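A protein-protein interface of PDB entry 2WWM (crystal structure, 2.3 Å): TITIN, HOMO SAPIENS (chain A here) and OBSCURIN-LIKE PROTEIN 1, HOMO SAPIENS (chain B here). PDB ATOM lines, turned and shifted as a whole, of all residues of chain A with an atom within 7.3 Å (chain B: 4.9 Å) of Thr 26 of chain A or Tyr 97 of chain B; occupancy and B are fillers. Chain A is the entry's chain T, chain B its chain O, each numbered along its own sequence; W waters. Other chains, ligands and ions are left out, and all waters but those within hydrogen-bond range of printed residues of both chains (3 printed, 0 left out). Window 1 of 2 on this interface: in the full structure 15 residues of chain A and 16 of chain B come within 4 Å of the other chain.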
ATOM      1  N   LEU A  13       8.059  27.058  10.501  1.00  0.00           N
ATOM      2  CA  LEU A  13       8.372  26.925   9.077  1.00  0.00           C
ATOM      3  C   LEU A  13       9.369  25.782   8.994  1.00  0.00           C
ATOM      4  O   LEU A  13      10.264  25.714   9.821  1.00  0.00           O
ATOM      5  CB  LEU A  13       8.990  28.210   8.515  1.00  0.00           C
ATOM      6  CG  LEU A  13       9.343  28.252   7.017  1.00  0.00           C
ATOM      7  CD1 LEU A  13       8.103  28.189   6.147  1.00  0.00           C
ATOM      8  CD2 LEU A  13      10.197  29.511   6.651  1.00  0.00           C
ATOM      9  N   PRO A  14       9.211  24.864   8.024  1.00  0.00           N
ATOM     10  CA  PRO A  14      10.178  23.763   7.887  1.00  0.00           C
ATOM     11  C   PRO A  14      11.607  24.251   7.625  1.00  0.00           C
ATOM     12  O   PRO A  14      11.792  25.340   7.094  1.00  0.00           O
ATOM     13  CB  PRO A  14       9.660  22.988   6.665  1.00  0.00           C
ATOM     14  CG  PRO A  14       8.223  23.277   6.625  1.00  0.00           C
ATOM     15  CD  PRO A  14       8.069  24.695   7.107  1.00  0.00           C
ATOM     16  N   ASP A  16      14.046  22.223   5.886  1.00  0.00           N
ATOM     17  CA  ASP A  16      14.355  21.716   4.554  1.00  0.00           C
ATOM     18  C   ASP A  16      13.121  21.060   3.945  1.00  0.00           C
ATOM     19  O   ASP A  16      12.401  20.313   4.613  1.00  0.00           O
ATOM     20  CB  ASP A  16      15.477  20.676   4.593  1.00  0.00           C
ATOM     21  CG  ASP A  16      16.838  21.283   4.884  1.00  0.00           C
ATOM     22  OD1 ASP A  16      17.069  21.666   6.059  1.00  0.00           O
ATOM     23  OD2 ASP A  16      17.677  21.347   3.946  1.00  0.00           O
ATOM     24  N   ILE A  17      12.885  21.339   2.671  1.00  0.00           N
ATOM     25  CA  ILE A  17      11.868  20.639   1.916  1.00  0.00           C
ATOM     26  C   ILE A  17      12.391  20.245   0.539  1.00  0.00           C
ATOM     27  O   ILE A  17      13.283  20.899  -0.014  1.00  0.00           O
ATOM     28  CB  ILE A  17      10.557  21.460   1.811  1.00  0.00           C
ATOM     29  CG1 ILE A  17      10.692  22.644   0.860  1.00  0.00           C
ATOM     30  CG2 ILE A  17      10.135  21.965   3.171  1.00  0.00           C
ATOM     31  CD1 ILE A  17       9.431  23.483   0.793  1.00  0.00           C
ATOM     32  N   SER A  18      11.830  19.169   0.000  1.00  0.00           N
ATOM     33  CA  SER A  18      12.258  18.634  -1.284  1.00  0.00           C
ATOM     34  C   SER A  18      11.084  18.486  -2.244  1.00  0.00           C
ATOM     35  O   SER A  18       9.951  18.300  -1.817  1.00  0.00           O
ATOM     36  CB  SER A  18      12.957  17.297  -1.069  1.00  0.00           C
ATOM     37  OG  SER A  18      14.063  17.479  -0.191  1.00  0.00           O
ATOM     38  N   ILE A  19      11.365  18.609  -3.537  1.00  0.00           N
ATOM     39  CA  ILE A  19      10.349  18.427  -4.579  1.00  0.00           C
ATOM     40  C   ILE A  19      10.984  17.908  -5.883  1.00  0.00           C
ATOM     41  O   ILE A  19      12.103  18.277  -6.220  1.00  0.00           O
ATOM     42  CB  ILE A  19       9.569  19.726  -4.850  1.00  0.00           C
ATOM     43  CG1 ILE A  19       8.279  19.442  -5.619  1.00  0.00           C
ATOM     44  CG2 ILE A  19      10.409  20.732  -5.633  1.00  0.00           C
ATOM     45  CD1 ILE A  19       7.179  18.805  -4.790  1.00  0.00           C
ATOM     46  N   VAL A  24       4.338  20.273  -8.675  1.00  0.00           N
ATOM     47  CA  VAL A  24       3.911  21.437  -7.906  1.00  0.00           C
ATOM     48  C   VAL A  24       4.386  21.292  -6.465  1.00  0.00           C
ATOM     49  O   VAL A  24       4.251  20.226  -5.876  1.00  0.00           O
ATOM     50  CB  VAL A  24       2.373  21.592  -7.925  1.00  0.00           C
ATOM     51  CG1 VAL A  24       1.904  22.707  -6.977  1.00  0.00           C
ATOM     52  CG2 VAL A  24       1.889  21.844  -9.345  1.00  0.00           C
ATOM     53  N   LEU A  25       4.940  22.370  -5.915  1.00  0.00           N
ATOM     54  CA  LEU A  25       5.287  22.462  -4.502  1.00  0.00           C
ATOM     55  C   LEU A  25       4.433  23.508  -3.799  1.00  0.00           C
ATOM     56  O   LEU A  25       4.295  24.632  -4.279  1.00  0.00           O
ATOM     57  CB  LEU A  25       6.757  22.860  -4.342  1.00  0.00           C
ATOM     58  CG  LEU A  25       7.266  23.137  -2.922  1.00  0.00           C
ATOM     59  CD1 LEU A  25       7.122  21.884  -2.048  1.00  0.00           C
ATOM     60  CD2 LEU A  25       8.720  23.645  -2.956  1.00  0.00           C
ATOM     61  N   THR A  26       3.892  23.138  -2.644  1.00  0.00           N
ATOM     62  CA  THR A  26       3.192  24.068  -1.774  1.00  0.00           C
ATOM     63  C   THR A  26       3.816  24.068  -0.354  1.00  0.00           C
ATOM     64  O   THR A  26       4.078  22.995   0.230  1.00  0.00           O
ATOM     65  CB  THR A  26       1.712  23.680  -1.663  1.00  0.00           C
ATOM     66  OG1 THR A  26       1.083  23.797  -2.947  1.00  0.00           O
ATOM     67  CG2 THR A  26       0.979  24.583  -0.662  1.00  0.00           C
ATOM     68  N   VAL A  27       4.058  25.264   0.188  1.00  0.00           N
ATOM     69  CA  VAL A  27       4.492  25.425   1.575  1.00  0.00           C
ATOM     70  C   VAL A  27       3.639  26.505   2.223  1.00  0.00           C
ATOM     71  O   VAL A  27       3.511  27.624   1.716  1.00  0.00           O
ATOM     72  CB  VAL A  27       6.017  25.736   1.686  1.00  0.00           C
ATOM     73  CG1 VAL A  27       6.378  27.010   0.963  1.00  0.00           C
ATOM     74  CG2 VAL A  27       6.475  25.810   3.162  1.00  0.00           C
ATOM     75  N   ALA A  28       3.018  26.141   3.329  1.00  0.00           N
ATOM     76  CA  ALA A  28       2.092  27.006   4.031  1.00  0.00           C
ATOM     77  C   ALA A  28       2.747  27.361   5.336  1.00  0.00           C
ATOM     78  O   ALA A  28       3.450  26.531   5.913  1.00  0.00           O
ATOM     79  CB  ALA A  28       0.775  26.269   4.304  1.00  0.00           C
ATOM     80  N   CYS A  29       2.504  28.578   5.804  1.00  0.00           N
ATOM     81  CA  CYS A  29       3.064  29.056   7.058  1.00  0.00           C
ATOM     82  C   CYS A  29       2.117  30.019   7.765  1.00  0.00           C
ATOM     83  O   CYS A  29       1.635  30.993   7.169  1.00  0.00           O
ATOM     84  CB  CYS A  29       4.418  29.731   6.850  1.00  0.00           C
ATOM     85  SG  CYS A  29       5.318  29.990   8.443  1.00  0.00           S
ATOM     86  N   GLU A  59      -0.574  33.294  -1.807  1.00  0.00           N
ATOM     87  CA  GLU A  59      -1.888  33.569  -1.245  1.00  0.00           C
ATOM     88  C   GLU A  59      -1.754  33.868   0.249  1.00  0.00           C
ATOM     89  O   GLU A  59      -1.280  33.023   1.010  1.00  0.00           O
ATOM     90  CB  GLU A  59      -2.819  32.368  -1.435  1.00  0.00           C
ATOM     91  CG  GLU A  59      -2.962  31.844  -2.879  1.00  0.00           C
ATOM     92  CD  GLU A  59      -3.875  30.595  -2.972  1.00  0.00           C
ATOM     93  OE1 GLU A  59      -5.031  30.651  -2.477  1.00  0.00           O
ATOM     94  OE2 GLU A  59      -3.440  29.561  -3.537  1.00  0.00           O
ATOM     95  N   THR A  65       0.162  32.358   5.048  1.00  0.00           N
ATOM     96  CA  THR A  65       0.724  32.582   3.722  1.00  0.00           C
ATOM     97  C   THR A  65       0.950  31.219   3.085  1.00  0.00           C
ATOM     98  O   THR A  65       1.402  30.287   3.752  1.00  0.00           O
ATOM     99  CB  THR A  65       2.062  33.358   3.771  1.00  0.00           C
ATOM    100  OG1 THR A  65       2.565  33.564   2.438  1.00  0.00           O
ATOM    101  CG2 THR A  65       3.117  32.611   4.588  1.00  0.00           C
ATOM    102  N   THR A  66       0.636  31.088   1.803  1.00  0.00           N
ATOM    103  CA  THR A  66       0.938  29.855   1.070  1.00  0.00           C
ATOM    104  C   THR A  66       1.730  30.213  -0.168  1.00  0.00           C
ATOM    105  O   THR A  66       1.313  31.071  -0.935  1.00  0.00           O
ATOM    106  CB  THR A  66      -0.346  29.092   0.662  1.00  0.00           C
ATOM    107  OG1 THR A  66      -1.200  28.946   1.796  1.00  0.00           O
ATOM    108  CG2 THR A  66      -0.013  27.723   0.104  1.00  0.00           C
ATOM    109  N   LEU A  67       2.872  29.561  -0.343  1.00  0.00           N
ATOM    110  CA  LEU A  67       3.677  29.690  -1.555  1.00  0.00           C
ATOM    111  C   LEU A  67       3.477  28.446  -2.390  1.00  0.00           C
ATOM    112  O   LEU A  67       3.708  27.340  -1.903  1.00  0.00           O
ATOM    113  CB  LEU A  67       5.160  29.831  -1.219  1.00  0.00           C
ATOM    114  CG  LEU A  67       6.184  29.896  -2.365  1.00  0.00           C
ATOM    115  CD1 LEU A  67       5.920  31.084  -3.279  1.00  0.00           C
ATOM    116  CD2 LEU A  67       7.611  29.970  -1.827  1.00  0.00           C
ATOM    117  N   ILE A  68       3.043  28.642  -3.641  1.00  0.00           N
ATOM    118  CA  ILE A  68       2.878  27.569  -4.619  1.00  0.00           C
ATOM    119  C   ILE A  68       3.827  27.805  -5.809  1.00  0.00           C
ATOM    120  O   ILE A  68       3.773  28.858  -6.454  1.00  0.00           O
ATOM    121  CB  ILE A  68       1.425  27.487  -5.127  1.00  0.00           C
ATOM    122  CG1 ILE A  68       0.450  27.360  -3.945  1.00  0.00           C
ATOM    123  CG2 ILE A  68       1.255  26.317  -6.110  1.00  0.00           C
ATOM    124  CD1 ILE A  68      -0.976  26.999  -4.342  1.00  0.00           C
ATOM    125  N   ILE A  69       4.710  26.840  -6.070  1.00  0.00           N
ATOM    126  CA  ILE A  69       5.538  26.821  -7.282  1.00  0.00           C
ATOM    127  C   ILE A  69       5.112  25.674  -8.218  1.00  0.00           C
ATOM    128  O   ILE A  69       5.276  24.481  -7.894  1.00  0.00           O
ATOM    129  CB  ILE A  69       7.030  26.647  -6.958  1.00  0.00           C
ATOM    130  CG1 ILE A  69       7.442  27.502  -5.744  1.00  0.00           C
ATOM    131  CG2 ILE A  69       7.887  27.006  -8.181  1.00  0.00           C
ATOM    132  CD1 ILE A  69       8.924  27.341  -5.350  1.00  0.00           C
ATOM    133  N   VAL A  72       8.012  22.814 -11.260  1.00  0.00           N
ATOM    134  CA  VAL A  72       9.246  23.179 -10.578  1.00  0.00           C
ATOM    135  C   VAL A  72      10.462  22.865 -11.447  1.00  0.00           C
ATOM    136  O   VAL A  72      10.613  21.746 -11.950  1.00  0.00           O
ATOM    137  CB  VAL A  72       9.354  22.466  -9.195  1.00  0.00           C
ATOM    138  CG1 VAL A  72      10.746  22.569  -8.628  1.00  0.00           C
ATOM    139  CG2 VAL A  72       8.349  23.053  -8.203  1.00  0.00           C
ATOM    140  N   VAL A  95      13.631  28.526   4.704  1.00  0.00           N
ATOM    141  CA  VAL A  95      13.509  27.109   4.400  1.00  0.00           C
ATOM    142  C   VAL A  95      14.341  26.838   3.142  1.00  0.00           C
ATOM    143  O   VAL A  95      14.295  27.623   2.175  1.00  0.00           O
ATOM    144  CB  VAL A  95      12.065  26.688   4.143  1.00  0.00           C
ATOM    145  CG1 VAL A  95      11.382  27.668   3.154  1.00  0.00           C
ATOM    146  CG2 VAL A  95      12.011  25.227   3.607  1.00  0.00           C
ATOM    147  N   HIS A  98      14.911  21.970  -1.927  1.00  0.00           N
ATOM    148  CA  HIS A  98      15.782  21.097  -2.741  1.00  0.00           C
ATOM    149  C   HIS A  98      15.005  20.510  -3.912  1.00  0.00           C
ATOM    150  O   HIS A  98      13.882  20.023  -3.739  1.00  0.00           O
ATOM    151  CB  HIS A  98      16.329  19.923  -1.916  1.00  0.00           C
ATOM    152  CG  HIS A  98      17.008  20.325  -0.642  1.00  0.00           C
ATOM    153  ND1 HIS A  98      18.358  20.591  -0.568  1.00  0.00           N
ATOM    154  CD2 HIS A  98      16.526  20.479   0.614  1.00  0.00           C
ATOM    155  CE1 HIS A  98      18.678  20.904   0.675  1.00  0.00           C
ATOM    156  NE2 HIS A  98      17.583  20.847   1.412  1.00  0.00           N
ATOM    157  N   ARG A 100      14.856  17.484  -6.619  1.00  0.00           N
ATOM    158  CA  ARG A 100      15.396  16.130  -6.904  1.00  0.00           C
ATOM    159  C   ARG A 100      15.624  15.915  -8.398  1.00  0.00           C
ATOM    160  O   ARG A 100      14.670  15.868  -9.179  1.00  0.00           O
ATOM    161  CB  ARG A 100      14.467  15.027  -6.383  1.00  0.00           C
ATOM    162  CG  ARG A 100      14.252  15.044  -4.871  1.00  0.00           C
ATOM    163  CD  ARG A 100      13.541  13.772  -4.372  1.00  0.00           C
ATOM    164  NE  ARG A 100      12.861  14.004  -3.090  1.00  0.00           N
ATOM    165  CZ  ARG A 100      11.667  14.589  -2.938  1.00  0.00           C
ATOM    166  NH1 ARG A 100      10.964  15.030  -3.978  1.00  0.00           N
ATOM    167  NH2 ARG A 100      11.168  14.744  -1.724  1.00  0.00           N
ATOM    168  N   PRO B  15      -1.343  18.037  -3.722  1.00  0.00           N
ATOM    169  CA  PRO B  15      -1.733  18.168  -2.333  1.00  0.00           C
ATOM    170  C   PRO B  15      -1.865  19.604  -1.843  1.00  0.00           C
ATOM    171  O   PRO B  15      -1.104  20.471  -2.256  1.00  0.00           O
ATOM    172  CB  PRO B  15      -0.588  17.471  -1.569  1.00  0.00           C
ATOM    173  CG  PRO B  15       0.161  16.690  -2.581  1.00  0.00           C
ATOM    174  CD  PRO B  15      -0.006  17.434  -3.848  1.00  0.00           C
ATOM    175  N   PHE B  17      -3.655  21.953   1.896  1.00  0.00           N
ATOM    176  CA  PHE B  17      -4.257  21.831   3.220  1.00  0.00           C
ATOM    177  C   PHE B  17      -5.608  22.525   3.307  1.00  0.00           C
ATOM    178  O   PHE B  17      -5.693  23.745   3.163  1.00  0.00           O
ATOM    179  CB  PHE B  17      -3.305  22.360   4.307  1.00  0.00           C
ATOM    180  CG  PHE B  17      -2.017  21.571   4.421  1.00  0.00           C
ATOM    181  CD1 PHE B  17      -1.958  20.419   5.185  1.00  0.00           C
ATOM    182  CD2 PHE B  17      -0.871  21.985   3.765  1.00  0.00           C
ATOM    183  CE1 PHE B  17      -0.778  19.690   5.282  1.00  0.00           C
ATOM    184  CE2 PHE B  17       0.311  21.262   3.865  1.00  0.00           C
ATOM    185  CZ  PHE B  17       0.351  20.107   4.616  1.00  0.00           C
ATOM    186  N   GLU B  49       7.813  14.609   9.863  1.00  0.00           N
ATOM    187  CA  GLU B  49       9.249  14.748   9.961  1.00  0.00           C
ATOM    188  C   GLU B  49       9.557  15.633  11.150  1.00  0.00           C
ATOM    189  O   GLU B  49       8.784  16.536  11.483  1.00  0.00           O
ATOM    190  CB  GLU B  49       9.815  15.385   8.693  1.00  0.00           C
ATOM    191  CG  GLU B  49       9.429  14.689   7.391  1.00  0.00           C
ATOM    192  CD  GLU B  49      10.142  15.293   6.173  1.00  0.00           C
ATOM    193  OE1 GLU B  49      10.201  16.540   6.081  1.00  0.00           O
ATOM    194  OE2 GLU B  49      10.646  14.533   5.309  1.00  0.00           O
ATOM    195  N   VAL B  86       6.999  18.672  10.970  1.00  0.00           N
ATOM    196  CA  VAL B  86       6.610  18.993   9.612  1.00  0.00           C
ATOM    197  C   VAL B  86       5.722  17.902   9.047  1.00  0.00           C
ATOM    198  O   VAL B  86       6.057  16.722   9.107  1.00  0.00           O
ATOM    199  CB  VAL B  86       7.836  19.143   8.702  1.00  0.00           C
ATOM    200  CG1 VAL B  86       7.392  19.552   7.281  1.00  0.00           C
ATOM    201  CG2 VAL B  86       8.808  20.171   9.300  1.00  0.00           C
ATOM    202  N   CYS B  87       4.588  18.323   8.501  1.00  0.00           N
ATOM    203  CA  CYS B  87       3.682  17.449   7.780  1.00  0.00           C
ATOM    204  C   CYS B  87       3.935  17.532   6.293  1.00  0.00           C
ATOM    205  O   CYS B  87       3.820  18.604   5.688  1.00  0.00           O
ATOM    206  CB  CYS B  87       2.231  17.841   8.025  1.00  0.00           C
ATOM    207  SG  CYS B  87       1.163  16.784   7.086  1.00  0.00           S
ATOM    208  N   ARG B  88       4.255  16.385   5.711  1.00  0.00           N
ATOM    209  CA  ARG B  88       4.600  16.307   4.301  1.00  0.00           C
ATOM    210  C   ARG B  88       3.595  15.415   3.607  1.00  0.00           C
ATOM    211  O   ARG B  88       3.498  14.232   3.918  1.00  0.00           O
ATOM    212  CB  ARG B  88       6.029  15.782   4.125  1.00  0.00           C
ATOM    213  CG  ARG B  88       6.393  15.463   2.691  1.00  0.00           C
ATOM    214  CD  ARG B  88       7.810  14.968   2.609  1.00  0.00           C
ATOM    215  NE  ARG B  88       8.066  14.318   1.337  1.00  0.00           N
ATOM    216  CZ  ARG B  88       9.230  13.795   0.967  1.00  0.00           C
ATOM    217  NH1 ARG B  88      10.297  13.843   1.766  1.00  0.00           N
ATOM    218  NH2 ARG B  88       9.324  13.221  -0.222  1.00  0.00           N
ATOM    219  N   GLU B  95       3.792  17.957  -3.868  1.00  0.00           N
ATOM    220  CA  GLU B  95       4.031  17.826  -2.431  1.00  0.00           C
ATOM    221  C   GLU B  95       3.606  19.097  -1.754  1.00  0.00           C
ATOM    222  O   GLU B  95       3.747  20.171  -2.312  1.00  0.00           O
ATOM    223  CB  GLU B  95       5.514  17.554  -2.122  1.00  0.00           C
ATOM    224  CG  GLU B  95       5.877  16.087  -2.087  1.00  0.00           C
ATOM    225  CD  GLU B  95       7.372  15.826  -1.959  1.00  0.00           C
ATOM    226  OE1 GLU B  95       7.957  15.209  -2.877  1.00  0.00           O
ATOM    227  OE2 GLU B  95       7.965  16.230  -0.939  1.00  0.00           O
ATOM    228  N   ALA B  96       3.075  18.964  -0.550  1.00  0.00           N
ATOM    229  CA  ALA B  96       2.727  20.112   0.283  1.00  0.00           C
ATOM    230  C   ALA B  96       3.330  19.973   1.671  1.00  0.00           C
ATOM    231  O   ALA B  96       3.361  18.885   2.239  1.00  0.00           O
ATOM    232  CB  ALA B  96       1.229  20.237   0.378  1.00  0.00           C
ATOM    233  N   TYR B  97       3.797  21.079   2.227  1.00  0.00           N
ATOM    234  CA  TYR B  97       4.452  21.066   3.530  1.00  0.00           C
ATOM    235  C   TYR B  97       3.820  22.122   4.439  1.00  0.00           C
ATOM    236  O   TYR B  97       3.475  23.227   3.996  1.00  0.00           O
ATOM    237  CB  TYR B  97       5.950  21.363   3.403  1.00  0.00           C
ATOM    238  CG  TYR B  97       6.823  20.295   2.747  1.00  0.00           C
ATOM    239  CD1 TYR B  97       7.678  19.489   3.508  1.00  0.00           C
ATOM    240  CD2 TYR B  97       6.837  20.131   1.371  1.00  0.00           C
ATOM    241  CE1 TYR B  97       8.494  18.527   2.906  1.00  0.00           C
ATOM    242  CE2 TYR B  97       7.633  19.183   0.768  1.00  0.00           C
ATOM    243  CZ  TYR B  97       8.459  18.382   1.530  1.00  0.00           C
ATOM    244  OH  TYR B  97       9.247  17.466   0.898  1.00  0.00           O
ATOM    245  N   ALA B  98       3.691  21.767   5.710  1.00  0.00           N
ATOM    246  CA  ALA B  98       3.220  22.663   6.748  1.00  0.00           C
ATOM    247  C   ALA B  98       3.866  22.217   8.045  1.00  0.00           C
ATOM    248  O   ALA B  98       4.103  20.999   8.236  1.00  0.00           O
ATOM    249  CB  ALA B  98       1.740  22.584   6.864  1.00  0.00           C
ATOM    250  N   ALA B  99       4.154  23.179   8.919  1.00  0.00           N
ATOM    251  CA  ALA B  99       4.797  22.901  10.204  1.00  0.00           C
ATOM    252  C   ALA B  99       3.947  23.352  11.402  1.00  0.00           C
ATOM    253  O   ALA B  99       3.075  24.219  11.264  1.00  0.00           O
ATOM    254  CB  ALA B  99       6.150  23.557  10.253  1.00  0.00           C
HETATM  255  O   HOH W   1       1.201  20.885  -3.732  1.00  0.00           O
HETATM  256  O   HOH W   2      10.650  18.801   6.910  1.00  0.00           O
HETATM  257  O   HOH W   3       4.776  25.862   7.809  1.00  0.00           O
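The backbone carbonyl oxygen (O) of Ser 18 of chain A sits close to the side-chain carboxylate (OE2) of Glu 95 of chain B (3.0 Å). OE1 of Glu 95 of chain B is in salt-bridge range of NH1 of Arg 100 of chain A (3.2 Å). The backbone carbonyl oxygen of Ser 18 of chain A sits at hydrogen-bond distance from the side-chain hydroxyl of Tyr 97 of chain B (2.9 Å). The backbone NH of Glu 95 of chain B is in hydrogen-bond range of the backbone carbonyl oxygen of Val 24 of chain A, 3.1 Å away. N of Tyr 97 of chain B sits at hydrogen-bond distance from O of Thr 26 of chain A, at 2.8 Å. The backbone carbonyl oxygen (O) of Tyr 97 of chain B lies within hydrogen-bond range of the backbone NH (N) of Ala 28 of chain A, at 3.0 Å. The backbone carbonyl oxygen (O) of Glu 95 of chain B lies within hydrogen-bond range of the backbone NH (N) of Thr 26 of chain A (3.0 Å). NH2 of Arg 100 of chain A sits close to NH2 of Arg 88 of chain B (2.8 Å).
NE of Arg 88 of chain B sits close to OH of Tyr 97 of chain B (3.4 Å). The backbone carbonyl oxygen (O) of His 98 of chain A lies within hydrogen-bond range of the backbone NH (N) of Ile 19 of chain A. NH1 of Arg 88 of chain B lies within salt-bridge range of OE2 of Glu 49 of chain B (3.6 Å). O of Ile 17 of chain A is in hydrogen-bond range of N of His 98 of chain A, 2.7 Å away. N of Ile 69 of chain A sits at hydrogen-bond distance from O of Leu 25 of chain A, at 2.9 Å. OE2 of Glu 95 of chain B lies within hydrogen-bond range of OH of Tyr 97 of chain B (2.6 Å).
Leu 13 of chain A touches Ala 99 of chain B (N to CB, 3.995 Å). Pro 14 of chain A touches Val 86 of chain B (CG to CG1, 3.9 Å). Pro 14 of chain A touches Ala 99 of chain B (CD to CB, 3.9 Å). Ile 17 of chain A touches Tyr 97 of chain B (CG2 to CD1, 3.5 Å). Glu 95 of chain B touches Ile 19 of chain A. Glu 95 of chain B touches Leu 25 of chain A (O to CA, 3.5 Å). Leu 25 of chain A touches Tyr 97 of chain B. Thr 26 of chain A touches Ala 96 of chain B (O to CA, 3.2 Å). Tyr 97 of chain B touches Val 27 of chain A. O of Ala 28 of chain A touches CA of Ala 98 of chain B, 3.96 Å away.
Of the printed residues of chain B, Leu 13 of chain A touches Ala 99 (3.995 Å). Of the printed residues of chain B, Ser 18 of chain A touches Glu 95 (3.0 Å) and Tyr 97 (2.9 Å). Of the printed residues of chain B, Leu 25 of chain A touches Glu 95 (3.5 Å) and Tyr 97 (3.9 Å). Thr 26 of chain A touches three residues of chain B. Of the printed residues of chain A, Ala 96 of chain B touches Thr 26. Of chain A, only Ile 17 (3.5 Å), Ser 18 (2.9 Å), Leu 25 (3.9 Å), Thr 26 (2.8 Å), Val 27 (3.4 Å) and Ala 28 (3.0 Å) come within 4 Å of Tyr 97 of chain B. The nearest residue of chain A that does not touch Tyr 97 of chain B is Arg 100 of chain A (4.2 Å). The nearest printed residue of chain A that does not touch Arg 88 of chain B is Ser 18 of chain A (5.2 Å).
Hydrophobic or aromatic side chains of chain A that line the printed part of chain B: Pro 14, Ile 17, Ile 19 and Leu 25. Along chain A the printed residues that touch a printed residue of chain B span positions 13 to 100. Hydrophobic or aromatic side chains of chain B within 4 Å of the printed part of chain A: Val 86, Ala 96, Tyr 97 and Ala 99. Among the printed residues, 18 pairs touch across the chains. Among the printed residues, Asp or Glu carboxylates within 4 Å of a Lys or Arg side-chain nitrogen of the other chain: Arg 100 of chain A with Glu 95 of chain B (3.2 Å).
Water W3 bridges O of Ala 28 of chain A (2.4 Å) and N of Ala 99 of chain B (3.0 Å). Water W2 lies within hydrogen-bond range of OE1 of Glu 49 of chain B (2.4 Å) and O of Asp 16 of chain A (3.3 Å). Water W1 lies within hydrogen-bond range of O of Pro 15 of chain B (2.8 Å), O of Glu 95 of chain B (3.0 Å) and OG1 of Thr 26 of chain A (3.0 Å).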
